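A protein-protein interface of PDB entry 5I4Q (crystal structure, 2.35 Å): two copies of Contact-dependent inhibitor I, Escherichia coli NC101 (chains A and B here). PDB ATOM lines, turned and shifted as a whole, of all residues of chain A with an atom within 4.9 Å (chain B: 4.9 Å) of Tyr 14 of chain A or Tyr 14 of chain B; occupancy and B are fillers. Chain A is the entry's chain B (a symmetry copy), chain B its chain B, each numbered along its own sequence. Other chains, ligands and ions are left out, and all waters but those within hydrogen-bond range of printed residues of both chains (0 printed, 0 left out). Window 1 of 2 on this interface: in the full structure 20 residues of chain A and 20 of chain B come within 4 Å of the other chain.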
ATOM      1  N   ASP A  10     -13.296  -6.840   9.425  1.00  0.00           N
ATOM      2  CA  ASP A  10     -14.436  -7.683   9.677  1.00  0.00           C
ATOM      3  C   ASP A  10     -15.583  -7.385   8.693  1.00  0.00           C
ATOM      4  O   ASP A  10     -16.255  -8.300   8.212  1.00  0.00           O
ATOM      5  CB  ASP A  10     -14.998  -7.427  11.083  1.00  0.00           C
ATOM      6  CG  ASP A  10     -14.126  -8.008  12.240  1.00  0.00           C
ATOM      7  OD1 ASP A  10     -13.146  -8.745  12.003  1.00  0.00           O
ATOM      8  OD2 ASP A  10     -14.456  -7.692  13.426  1.00  0.00           O
ATOM      9  N   LEU A  11     -15.832  -6.103   8.425  1.00  0.00           N
ATOM     10  CA  LEU A  11     -16.880  -5.716   7.536  1.00  0.00           C
ATOM     11  C   LEU A  11     -16.656  -6.166   6.094  1.00  0.00           C
ATOM     12  O   LEU A  11     -17.561  -6.636   5.414  1.00  0.00           O
ATOM     13  CB  LEU A  11     -17.088  -4.211   7.623  1.00  0.00           C
ATOM     14  CG  LEU A  11     -17.770  -3.838   8.914  1.00  0.00           C
ATOM     15  CD1 LEU A  11     -17.735  -2.318   9.046  1.00  0.00           C
ATOM     16  CD2 LEU A  11     -19.192  -4.344   8.894  1.00  0.00           C
ATOM     17  N   GLU A  12     -15.434  -6.098   5.659  1.00  0.00           N
ATOM     18  CA  GLU A  12     -15.033  -6.590   4.348  1.00  0.00           C
ATOM     19  C   GLU A  12     -15.219  -8.112   4.237  1.00  0.00           C
ATOM     20  O   GLU A  12     -15.710  -8.611   3.231  1.00  0.00           O
ATOM     21  CB  GLU A  12     -13.563  -6.216   4.198  1.00  0.00           C
ATOM     22  CG  GLU A  12     -13.004  -6.391   2.823  1.00  0.00           C
ATOM     23  CD  GLU A  12     -11.651  -5.702   2.640  1.00  0.00           C
ATOM     24  OE1 GLU A  12     -11.203  -4.942   3.551  1.00  0.00           O
ATOM     25  OE2 GLU A  12     -11.058  -5.925   1.550  1.00  0.00           O
ATOM     26  N   MET A  13     -14.834  -8.832   5.291  1.00  0.00           N
ATOM     27  CA  MET A  13     -15.060 -10.273   5.439  1.00  0.00           C
ATOM     28  C   MET A  13     -16.540 -10.560   5.440  1.00  0.00           C
ATOM     29  O   MET A  13     -16.983 -11.455   4.794  1.00  0.00           O
ATOM     30  CB  MET A  13     -14.425 -10.692   6.770  1.00  0.00           C
ATOM     31  CG  MET A  13     -13.771 -12.073   6.944  1.00  0.00           C
ATOM     32  SD  MET A  13     -12.359 -12.015   8.404  1.00  0.00           S
ATOM     33  CE  MET A  13     -11.049 -10.630   7.847  1.00  0.00           C
ATOM     34  N   TYR A  14     -17.338  -9.764   6.148  1.00  0.00           N
ATOM     35  CA  TYR A  14     -18.781  -9.953   6.131  1.00  0.00           C
ATOM     36  C   TYR A  14     -19.351  -9.810   4.694  1.00  0.00           C
ATOM     37  O   TYR A  14     -20.081 -10.678   4.190  1.00  0.00           O
ATOM     38  CB  TYR A  14     -19.444  -9.000   7.100  1.00  0.00           C
ATOM     39  CG  TYR A  14     -20.947  -8.983   7.031  1.00  0.00           C
ATOM     40  CD1 TYR A  14     -21.696  -9.846   7.809  1.00  0.00           C
ATOM     41  CD2 TYR A  14     -21.628  -8.088   6.165  1.00  0.00           C
ATOM     42  CE1 TYR A  14     -23.062  -9.842   7.759  1.00  0.00           C
ATOM     43  CE2 TYR A  14     -23.005  -8.083   6.096  1.00  0.00           C
ATOM     44  CZ  TYR A  14     -23.725  -8.965   6.899  1.00  0.00           C
ATOM     45  OH  TYR A  14     -25.094  -8.960   6.916  1.00  0.00           O
ATOM     46  N   ARG A  15     -18.937  -8.760   4.007  1.00  0.00           N
ATOM     47  CA  ARG A  15     -19.402  -8.537   2.644  1.00  0.00           C
ATOM     48  C   ARG A  15     -19.049  -9.726   1.744  1.00  0.00           C
ATOM     49  O   ARG A  15     -19.853 -10.165   0.982  1.00  0.00           O
ATOM     50  CB  ARG A  15     -18.794  -7.269   2.074  1.00  0.00           C
ATOM     51  CG  ARG A  15     -19.350  -6.983   0.666  1.00  0.00           C
ATOM     52  CD  ARG A  15     -18.444  -6.135  -0.172  1.00  0.00           C
ATOM     53  NE  ARG A  15     -17.141  -6.754  -0.239  1.00  0.00           N
ATOM     54  CZ  ARG A  15     -16.008  -6.073  -0.262  1.00  0.00           C
ATOM     55  NH1 ARG A  15     -16.017  -4.749  -0.226  1.00  0.00           N
ATOM     56  NH2 ARG A  15     -14.858  -6.728  -0.287  1.00  0.00           N
ATOM     57  N   ASP A  16     -17.828 -10.219   1.839  1.00  0.00           N
ATOM     58  CA  ASP A  16     -17.392 -11.319   1.010  1.00  0.00           C
ATOM     59  C   ASP A  16     -18.096 -12.633   1.315  1.00  0.00           C
ATOM     60  O   ASP A  16     -18.462 -13.355   0.410  1.00  0.00           O
ATOM     61  CB  ASP A  16     -15.896 -11.501   1.114  1.00  0.00           C
ATOM     62  CG  ASP A  16     -15.112 -10.311   0.538  1.00  0.00           C
ATOM     63  OD1 ASP A  16     -15.695  -9.491  -0.192  1.00  0.00           O
ATOM     64  OD2 ASP A  16     -13.894 -10.181   0.810  1.00  0.00           O
ATOM     65  N   VAL A  17     -18.301 -12.946   2.570  1.00  0.00           N
ATOM     66  CA  VAL A  17     -18.929 -14.192   2.888  1.00  0.00           C
ATOM     67  C   VAL A  17     -20.407 -14.201   2.547  1.00  0.00           C
ATOM     68  O   VAL A  17     -20.908 -15.207   2.023  1.00  0.00           O
ATOM     69  CB  VAL A  17     -18.634 -14.694   4.323  1.00  0.00           C
ATOM     70  CG1 VAL A  17     -19.506 -14.055   5.370  1.00  0.00           C
ATOM     71  CG2 VAL A  17     -18.854 -16.172   4.366  1.00  0.00           C
ATOM     72  N   VAL A  18     -21.080 -13.087   2.759  1.00  0.00           N
ATOM     73  CA  VAL A  18     -22.498 -12.988   2.442  1.00  0.00           C
ATOM     74  C   VAL A  18     -22.700 -13.122   0.934  1.00  0.00           C
ATOM     75  O   VAL A  18     -23.568 -13.819   0.464  1.00  0.00           O
ATOM     76  CB  VAL A  18     -23.061 -11.682   3.008  1.00  0.00           C
ATOM     77  CG1 VAL A  18     -24.396 -11.301   2.417  1.00  0.00           C
ATOM     78  CG2 VAL A  18     -23.199 -11.815   4.514  1.00  0.00           C
ATOM     79  N   LEU A  19     -21.865 -12.450   0.166  1.00  0.00           N
ATOM     80  CA  LEU A  19     -21.905 -12.571  -1.288  1.00  0.00           C
ATOM     81  C   LEU A  19     -21.864 -14.026  -1.709  1.00  0.00           C
ATOM     82  O   LEU A  19     -22.621 -14.452  -2.595  1.00  0.00           O
ATOM     83  CB  LEU A  19     -20.702 -11.864  -1.857  1.00  0.00           C
ATOM     84  CG  LEU A  19     -20.554 -11.705  -3.330  1.00  0.00           C
ATOM     85  CD1 LEU A  19     -21.715 -10.889  -3.870  1.00  0.00           C
ATOM     86  CD2 LEU A  19     -19.252 -10.978  -3.604  1.00  0.00           C
ATOM     87  N   ILE A  21     -22.436 -16.838   0.227  1.00  0.00           N
ATOM     88  CA  ILE A  21     -23.571 -17.587   0.738  1.00  0.00           C
ATOM     89  C   ILE A  21     -24.773 -17.399  -0.167  1.00  0.00           C
ATOM     90  O   ILE A  21     -25.456 -18.359  -0.458  1.00  0.00           O
ATOM     91  CB  ILE A  21     -23.891 -17.166   2.185  1.00  0.00           C
ATOM     92  CG1 ILE A  21     -22.828 -17.720   3.106  1.00  0.00           C
ATOM     93  CG2 ILE A  21     -25.281 -17.604   2.627  1.00  0.00           C
ATOM     94  CD1 ILE A  21     -22.817 -17.005   4.452  1.00  0.00           C
ATOM     95  N   TYR A  68     -26.059 -21.945  12.319  1.00  0.00           N
ATOM     96  CA  TYR A  68     -25.187 -20.837  11.995  1.00  0.00           C
ATOM     97  C   TYR A  68     -25.945 -19.527  11.970  1.00  0.00           C
ATOM     98  O   TYR A  68     -25.353 -18.518  11.821  1.00  0.00           O
ATOM     99  CB  TYR A  68     -24.502 -21.084  10.645  1.00  0.00           C
ATOM    100  CG  TYR A  68     -23.660 -22.289  10.704  1.00  0.00           C
ATOM    101  CD1 TYR A  68     -22.454 -22.257  11.354  1.00  0.00           C
ATOM    102  CD2 TYR A  68     -24.086 -23.476  10.146  1.00  0.00           C
ATOM    103  CE1 TYR A  68     -21.711 -23.390  11.509  1.00  0.00           C
ATOM    104  CE2 TYR A  68     -23.322 -24.596  10.248  1.00  0.00           C
ATOM    105  CZ  TYR A  68     -22.154 -24.543  10.947  1.00  0.00           C
ATOM    106  OH  TYR A  68     -21.383 -25.649  11.047  1.00  0.00           O
ATOM    107  N   GLU A  69     -27.252 -19.587  12.022  1.00  0.00           N
ATOM    108  CA  GLU A  69     -28.110 -18.403  12.096  1.00  0.00           C
ATOM    109  C   GLU A  69     -28.028 -17.490  10.895  1.00  0.00           C
ATOM    110  O   GLU A  69     -28.060 -16.281  11.027  1.00  0.00           O
ATOM    111  CB  GLU A  69     -27.914 -17.674  13.437  1.00  0.00           C
ATOM    112  CG  GLU A  69     -28.466 -18.569  14.565  1.00  0.00           C
ATOM    113  CD  GLU A  69     -28.370 -17.911  15.932  1.00  0.00           C
ATOM    114  OE1 GLU A  69     -27.254 -17.782  16.437  1.00  0.00           O
ATOM    115  OE2 GLU A  69     -29.423 -17.499  16.480  1.00  0.00           O
ATOM    116  N   TYR A  70     -27.881 -18.081   9.716  1.00  0.00           N
ATOM    117  CA  TYR A  70     -28.008 -17.308   8.499  1.00  0.00           C
ATOM    118  C   TYR A  70     -29.465 -17.362   8.101  1.00  0.00           C
ATOM    119  O   TYR A  70     -30.012 -18.425   7.838  1.00  0.00           O
ATOM    120  CB  TYR A  70     -27.075 -17.764   7.383  1.00  0.00           C
ATOM    121  CG  TYR A  70     -27.181 -16.811   6.180  1.00  0.00           C
ATOM    122  CD1 TYR A  70     -28.210 -16.940   5.243  1.00  0.00           C
ATOM    123  CD2 TYR A  70     -26.291 -15.756   6.034  1.00  0.00           C
ATOM    124  CE1 TYR A  70     -28.316 -16.051   4.189  1.00  0.00           C
ATOM    125  CE2 TYR A  70     -26.406 -14.856   4.979  1.00  0.00           C
ATOM    126  CZ  TYR A  70     -27.415 -15.015   4.067  1.00  0.00           C
ATOM    127  OH  TYR A  70     -27.535 -14.132   3.085  1.00  0.00           O
ATOM    128  N   ASP B  10     -18.093 -21.411   4.976  1.00  0.00           N
ATOM    129  CA  ASP B  10     -18.587 -20.066   4.838  1.00  0.00           C
ATOM    130  C   ASP B  10     -19.567 -19.709   5.972  1.00  0.00           C
ATOM    131  O   ASP B  10     -19.544 -18.594   6.498  1.00  0.00           O
ATOM    132  CB  ASP B  10     -19.369 -19.908   3.527  1.00  0.00           C
ATOM    133  CG  ASP B  10     -18.478 -19.870   2.246  1.00  0.00           C
ATOM    134  OD1 ASP B  10     -17.233 -19.817   2.327  1.00  0.00           O
ATOM    135  OD2 ASP B  10     -19.076 -19.900   1.125  1.00  0.00           O
ATOM    136  N   LEU B  11     -20.455 -20.641   6.319  1.00  0.00           N
ATOM    137  CA  LEU B  11     -21.416 -20.410   7.349  1.00  0.00           C
ATOM    138  C   LEU B  11     -20.798 -20.219   8.732  1.00  0.00           C
ATOM    139  O   LEU B  11     -21.189 -19.350   9.502  1.00  0.00           O
ATOM    140  CB  LEU B  11     -22.440 -21.535   7.348  1.00  0.00           C
ATOM    141  CG  LEU B  11     -23.372 -21.411   6.170  1.00  0.00           C
ATOM    142  CD1 LEU B  11     -24.211 -22.684   6.094  1.00  0.00           C
ATOM    143  CD2 LEU B  11     -24.251 -20.198   6.351  1.00  0.00           C
ATOM    144  N   GLU B  12     -19.779 -20.976   9.010  1.00  0.00           N
ATOM    145  CA  GLU B  12     -19.009 -20.845  10.239  1.00  0.00           C
ATOM    146  C   GLU B  12     -18.294 -19.485  10.313  1.00  0.00           C
ATOM    147  O   GLU B  12     -18.289 -18.838  11.353  1.00  0.00           O
ATOM    148  CB  GLU B  12     -17.995 -21.984  10.215  1.00  0.00           C
ATOM    149  CG  GLU B  12     -17.264 -22.206  11.499  1.00  0.00           C
ATOM    150  CD  GLU B  12     -16.519 -23.540  11.535  1.00  0.00           C
ATOM    151  OE1 GLU B  12     -16.694 -24.385  10.605  1.00  0.00           O
ATOM    152  OE2 GLU B  12     -15.770 -23.731  12.532  1.00  0.00           O
ATOM    153  N   MET B  13     -17.710 -19.064   9.191  1.00  0.00           N
ATOM    154  CA  MET B  13     -17.107 -17.739   9.016  1.00  0.00           C
ATOM    155  C   MET B  13     -18.159 -16.673   9.192  1.00  0.00           C
ATOM    156  O   MET B  13     -17.938 -15.710   9.854  1.00  0.00           O
ATOM    157  CB  MET B  13     -16.523 -17.695   7.600  1.00  0.00           C
ATOM    158  CG  MET B  13     -15.236 -16.912   7.290  1.00  0.00           C
ATOM    159  SD  MET B  13     -14.299 -17.693   5.665  1.00  0.00           S
ATOM    160  CE  MET B  13     -13.930 -19.594   6.105  1.00  0.00           C
ATOM    161  N   TYR B  14     -19.348 -16.857   8.624  1.00  0.00           N
ATOM    162  CA  TYR B  14     -20.421 -15.893   8.817  1.00  0.00           C
ATOM    163  C   TYR B  14     -20.785 -15.749  10.319  1.00  0.00           C
ATOM    164  O   TYR B  14     -20.833 -14.642  10.879  1.00  0.00           O
ATOM    165  CB  TYR B  14     -21.621 -16.272   7.978  1.00  0.00           C
ATOM    166  CG  TYR B  14     -22.853 -15.448   8.239  1.00  0.00           C
ATOM    167  CD1 TYR B  14     -23.082 -14.284   7.530  1.00  0.00           C
ATOM    168  CD2 TYR B  14     -23.800 -15.841   9.219  1.00  0.00           C
ATOM    169  CE1 TYR B  14     -24.196 -13.525   7.754  1.00  0.00           C
ATOM    170  CE2 TYR B  14     -24.922 -15.078   9.463  1.00  0.00           C
ATOM    171  CZ  TYR B  14     -25.120 -13.913   8.725  1.00  0.00           C
ATOM    172  OH  TYR B  14     -26.246 -13.150   8.882  1.00  0.00           O
ATOM    173  N   ARG B  15     -20.946 -16.877  10.989  1.00  0.00           N
ATOM    174  CA  ARG B  15     -21.278 -16.854  12.408  1.00  0.00           C
ATOM    175  C   ARG B  15     -20.209 -16.103  13.208  1.00  0.00           C
ATOM    176  O   ARG B  15     -20.524 -15.320  14.049  1.00  0.00           O
ATOM    177  CB  ARG B  15     -21.418 -18.267  12.945  1.00  0.00           C
ATOM    178  CG  ARG B  15     -21.854 -18.247  14.423  1.00  0.00           C
ATOM    179  CD  ARG B  15     -21.479 -19.489  15.170  1.00  0.00           C
ATOM    180  NE  ARG B  15     -20.058 -19.709  15.047  1.00  0.00           N
ATOM    181  CZ  ARG B  15     -19.508 -20.908  14.952  1.00  0.00           C
ATOM    182  NH1 ARG B  15     -20.261 -21.998  14.970  1.00  0.00           N
ATOM    183  NH2 ARG B  15     -18.197 -21.011  14.804  1.00  0.00           N
ATOM    184  N   ASP B  16     -18.945 -16.375  12.939  1.00  0.00           N
ATOM    185  CA  ASP B  16     -17.867 -15.741  13.662  1.00  0.00           C
ATOM    186  C   ASP B  16     -17.746 -14.248  13.397  1.00  0.00           C
ATOM    187  O   ASP B  16     -17.526 -13.481  14.313  1.00  0.00           O
ATOM    188  CB  ASP B  16     -16.553 -16.425  13.361  1.00  0.00           C
ATOM    189  CG  ASP B  16     -16.504 -17.871  13.879  1.00  0.00           C
ATOM    190  OD1 ASP B  16     -17.348 -18.251  14.709  1.00  0.00           O
ATOM    191  OD2 ASP B  16     -15.614 -18.650  13.459  1.00  0.00           O
ATOM    192  N   VAL B  17     -17.899 -13.825  12.168  1.00  0.00           N
ATOM    193  CA  VAL B  17     -17.756 -12.429  11.884  1.00  0.00           C
ATOM    194  C   VAL B  17     -18.918 -11.608  12.410  1.00  0.00           C
ATOM    195  O   VAL B  17     -18.698 -10.515  12.953  1.00  0.00           O
ATOM    196  CB  VAL B  17     -17.416 -12.123  10.404  1.00  0.00           C
ATOM    197  CG1 VAL B  17     -18.621 -12.123   9.503  1.00  0.00           C
ATOM    198  CG2 VAL B  17     -16.774 -10.775  10.332  1.00  0.00           C
ATOM    199  N   VAL B  18     -20.119 -12.145  12.329  1.00  0.00           N
ATOM    200  CA  VAL B  18     -21.296 -11.445  12.828  1.00  0.00           C
ATOM    201  C   VAL B  18     -21.194 -11.281  14.342  1.00  0.00           C
ATOM    202  O   VAL B  18     -21.454 -10.236  14.892  1.00  0.00           O
ATOM    203  CB  VAL B  18     -22.560 -12.189  12.389  1.00  0.00           C
ATOM    204  CG1 VAL B  18     -23.791 -11.780  13.161  1.00  0.00           C
ATOM    205  CG2 VAL B  18     -22.790 -11.942  10.909  1.00  0.00           C
ATOM    206  N   LEU B  19     -20.788 -12.335  15.024  1.00  0.00           N
ATOM    207  CA  LEU B  19     -20.568 -12.269  16.465  1.00  0.00           C
ATOM    208  C   LEU B  19     -19.667 -11.104  16.821  1.00  0.00           C
ATOM    209  O   LEU B  19     -19.935 -10.363  17.778  1.00  0.00           O
ATOM    210  CB  LEU B  19     -19.906 -13.550  16.904  1.00  0.00           C
ATOM    211  CG  LEU B  19     -19.686 -13.822  18.350  1.00  0.00           C
ATOM    212  CD1 LEU B  19     -21.025 -13.868  19.066  1.00  0.00           C
ATOM    213  CD2 LEU B  19     -18.993 -15.163  18.485  1.00  0.00           C
ATOM    214  N   ILE B  21     -18.806  -8.380  14.864  1.00  0.00           N
ATOM    215  CA  ILE B  21     -19.382  -7.105  14.473  1.00  0.00           C
ATOM    216  C   ILE B  21     -20.356  -6.623  15.530  1.00  0.00           C
ATOM    217  O   ILE B  21     -20.340  -5.457  15.868  1.00  0.00           O
ATOM    218  CB  ILE B  21     -20.064  -7.218  13.096  1.00  0.00           C
ATOM    219  CG1 ILE B  21     -19.001  -7.318  12.026  1.00  0.00           C
ATOM    220  CG2 ILE B  21     -21.013  -6.060  12.818  1.00  0.00           C
ATOM    221  CD1 ILE B  21     -19.564  -7.863  10.718  1.00  0.00           C
ATOM    222  N   TYR B  68     -20.455  -1.650   3.141  1.00  0.00           N
ATOM    223  CA  TYR B  68     -20.320  -3.069   3.395  1.00  0.00           C
ATOM    224  C   TYR B  68     -21.672  -3.730   3.567  1.00  0.00           C
ATOM    225  O   TYR B  68     -21.732  -4.902   3.680  1.00  0.00           O
ATOM    226  CB  TYR B  68     -19.449  -3.301   4.636  1.00  0.00           C
ATOM    227  CG  TYR B  68     -18.093  -2.772   4.423  1.00  0.00           C
ATOM    228  CD1 TYR B  68     -17.206  -3.449   3.626  1.00  0.00           C
ATOM    229  CD2 TYR B  68     -17.706  -1.573   4.984  1.00  0.00           C
ATOM    230  CE1 TYR B  68     -15.983  -2.920   3.334  1.00  0.00           C
ATOM    231  CE2 TYR B  68     -16.466  -1.070   4.741  1.00  0.00           C
ATOM    232  CZ  TYR B  68     -15.629  -1.741   3.902  1.00  0.00           C
ATOM    233  OH  TYR B  68     -14.391  -1.253   3.661  1.00  0.00           O
ATOM    234  N   GLU B  69     -22.713  -2.946   3.681  1.00  0.00           N
ATOM    235  CA  GLU B  69     -24.089  -3.443   3.763  1.00  0.00           C
ATOM    236  C   GLU B  69     -24.380  -4.292   4.978  1.00  0.00           C
ATOM    237  O   GLU B  69     -25.100  -5.269   4.899  1.00  0.00           O
ATOM    238  CB  GLU B  69     -24.508  -4.104   2.437  1.00  0.00           C
ATOM    239  CG  GLU B  69     -24.602  -3.009   1.355  1.00  0.00           C
ATOM    240  CD  GLU B  69     -25.066  -3.554   0.013  1.00  0.00           C
ATOM    241  OE1 GLU B  69     -24.289  -4.266  -0.625  1.00  0.00           O
ATOM    242  OE2 GLU B  69     -26.228  -3.284  -0.379  1.00  0.00           O
ATOM    243  N   TYR B  70     -23.779  -3.931   6.105  1.00  0.00           N
ATOM    244  CA  TYR B  70     -24.160  -4.547   7.357  1.00  0.00           C
ATOM    245  C   TYR B  70     -25.272  -3.703   7.935  1.00  0.00           C
ATOM    246  O   TYR B  70     -25.091  -2.527   8.224  1.00  0.00           O
ATOM    247  CB  TYR B  70     -22.998  -4.736   8.326  1.00  0.00           C
ATOM    248  CG  TYR B  70     -23.465  -5.513   9.570  1.00  0.00           C
ATOM    249  CD1 TYR B  70     -24.116  -4.866  10.625  1.00  0.00           C
ATOM    250  CD2 TYR B  70     -23.309  -6.890   9.643  1.00  0.00           C
ATOM    251  CE1 TYR B  70     -24.566  -5.584  11.718  1.00  0.00           C
ATOM    252  CE2 TYR B  70     -23.773  -7.611  10.738  1.00  0.00           C
ATOM    253  CZ  TYR B  70     -24.393  -6.951  11.765  1.00  0.00           C
ATOM    254  OH  TYR B  70     -24.861  -7.653  12.787  1.00  0.00           O
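Asp 10 of chain A touches Val 17 of chain B.
Ile 21 of chain B touches Leu 11 of chain A.
Tyr 68 of chain B touches Leu 11 of chain A (CG to CB, 3.6 Å).
Tyr 68 of chain B touches Glu 12 of chain A (CD1 to N, 3.8 Å).
Tyr 14 of chain A touches Tyr 14 of chain B.
CE1 of Tyr 14 of chain A touches CG2 of Val 18 of chain B, at 3.8 Å.
Tyr 14 of chain A touches Tyr 70 of chain B (CZ to CD2, 3.5 Å).
CD1 of Ile 21 of chain A touches CD2 of Leu 11 of chain B (3.98 Å).
CD1 of Ile 21 of chain A touches CB of Tyr 14 of chain B, at 3.8 Å.
Tyr 70 of chain A touches Tyr 14 of chain B (CD2 to CZ, 3.5 Å).
Of the printed residues of chain B, Tyr 14 of chain A touches Tyr 14, Val 18, Ile 21, Glu 69 and Tyr 70.
Of the printed residues of chain B, Ile 21 of chain A touches Leu 11 and Tyr 14.
Of the printed residues of chain B, Tyr 68 of chain A touches Leu 11 and Glu 12.
Arg 15 of chain B touches none of the printed residues of chain A.
Of the printed residues of chain A, Val 18 of chain B touches Tyr 14.
The nearest printed residue of chain A that does not touch Tyr 14 of chain B is Val 17 of chain A (4.01 Å).
The nearest printed residue of chain A that does not touch Tyr 70 of chain B is Val 18 of chain A (7.1 Å).
Of the 14 printed residues of chain A, 10 touch a printed residue of chain B.
Hydrophobic or aromatic side chains of chain A that line the printed part of chain B: Leu 11, Tyr 14, Val 17, Val 18, Ile 21, Tyr 68 and Tyr 70.
Of the 14 printed residues of chain B, 10 touch a printed residue of chain A.
Among the printed residues, 19 pairs touch across the chains.
Leu 11 of chain A touches Ile 21 of chain B, and with the chains exchanged Ile 21 of chain A touches Leu 11 of chain B.
Leu 11 of chain A touches Tyr 68 of chain B, and with the chains exchanged Tyr 68 of chain A touches Leu 11 of chain B.
Tyr 14 of chain A touches its own counterpart, Tyr 14 of chain B.
Tyr 14 of chain A touches Ile 21 of chain B, and with the chains exchanged Ile 21 of chain A touches Tyr 14 of chain B.
Positions printed for both chains: 10, 11, 12, 13, 14, 15, 16, 17, 18, 19, 21, 68, 69 and 70.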
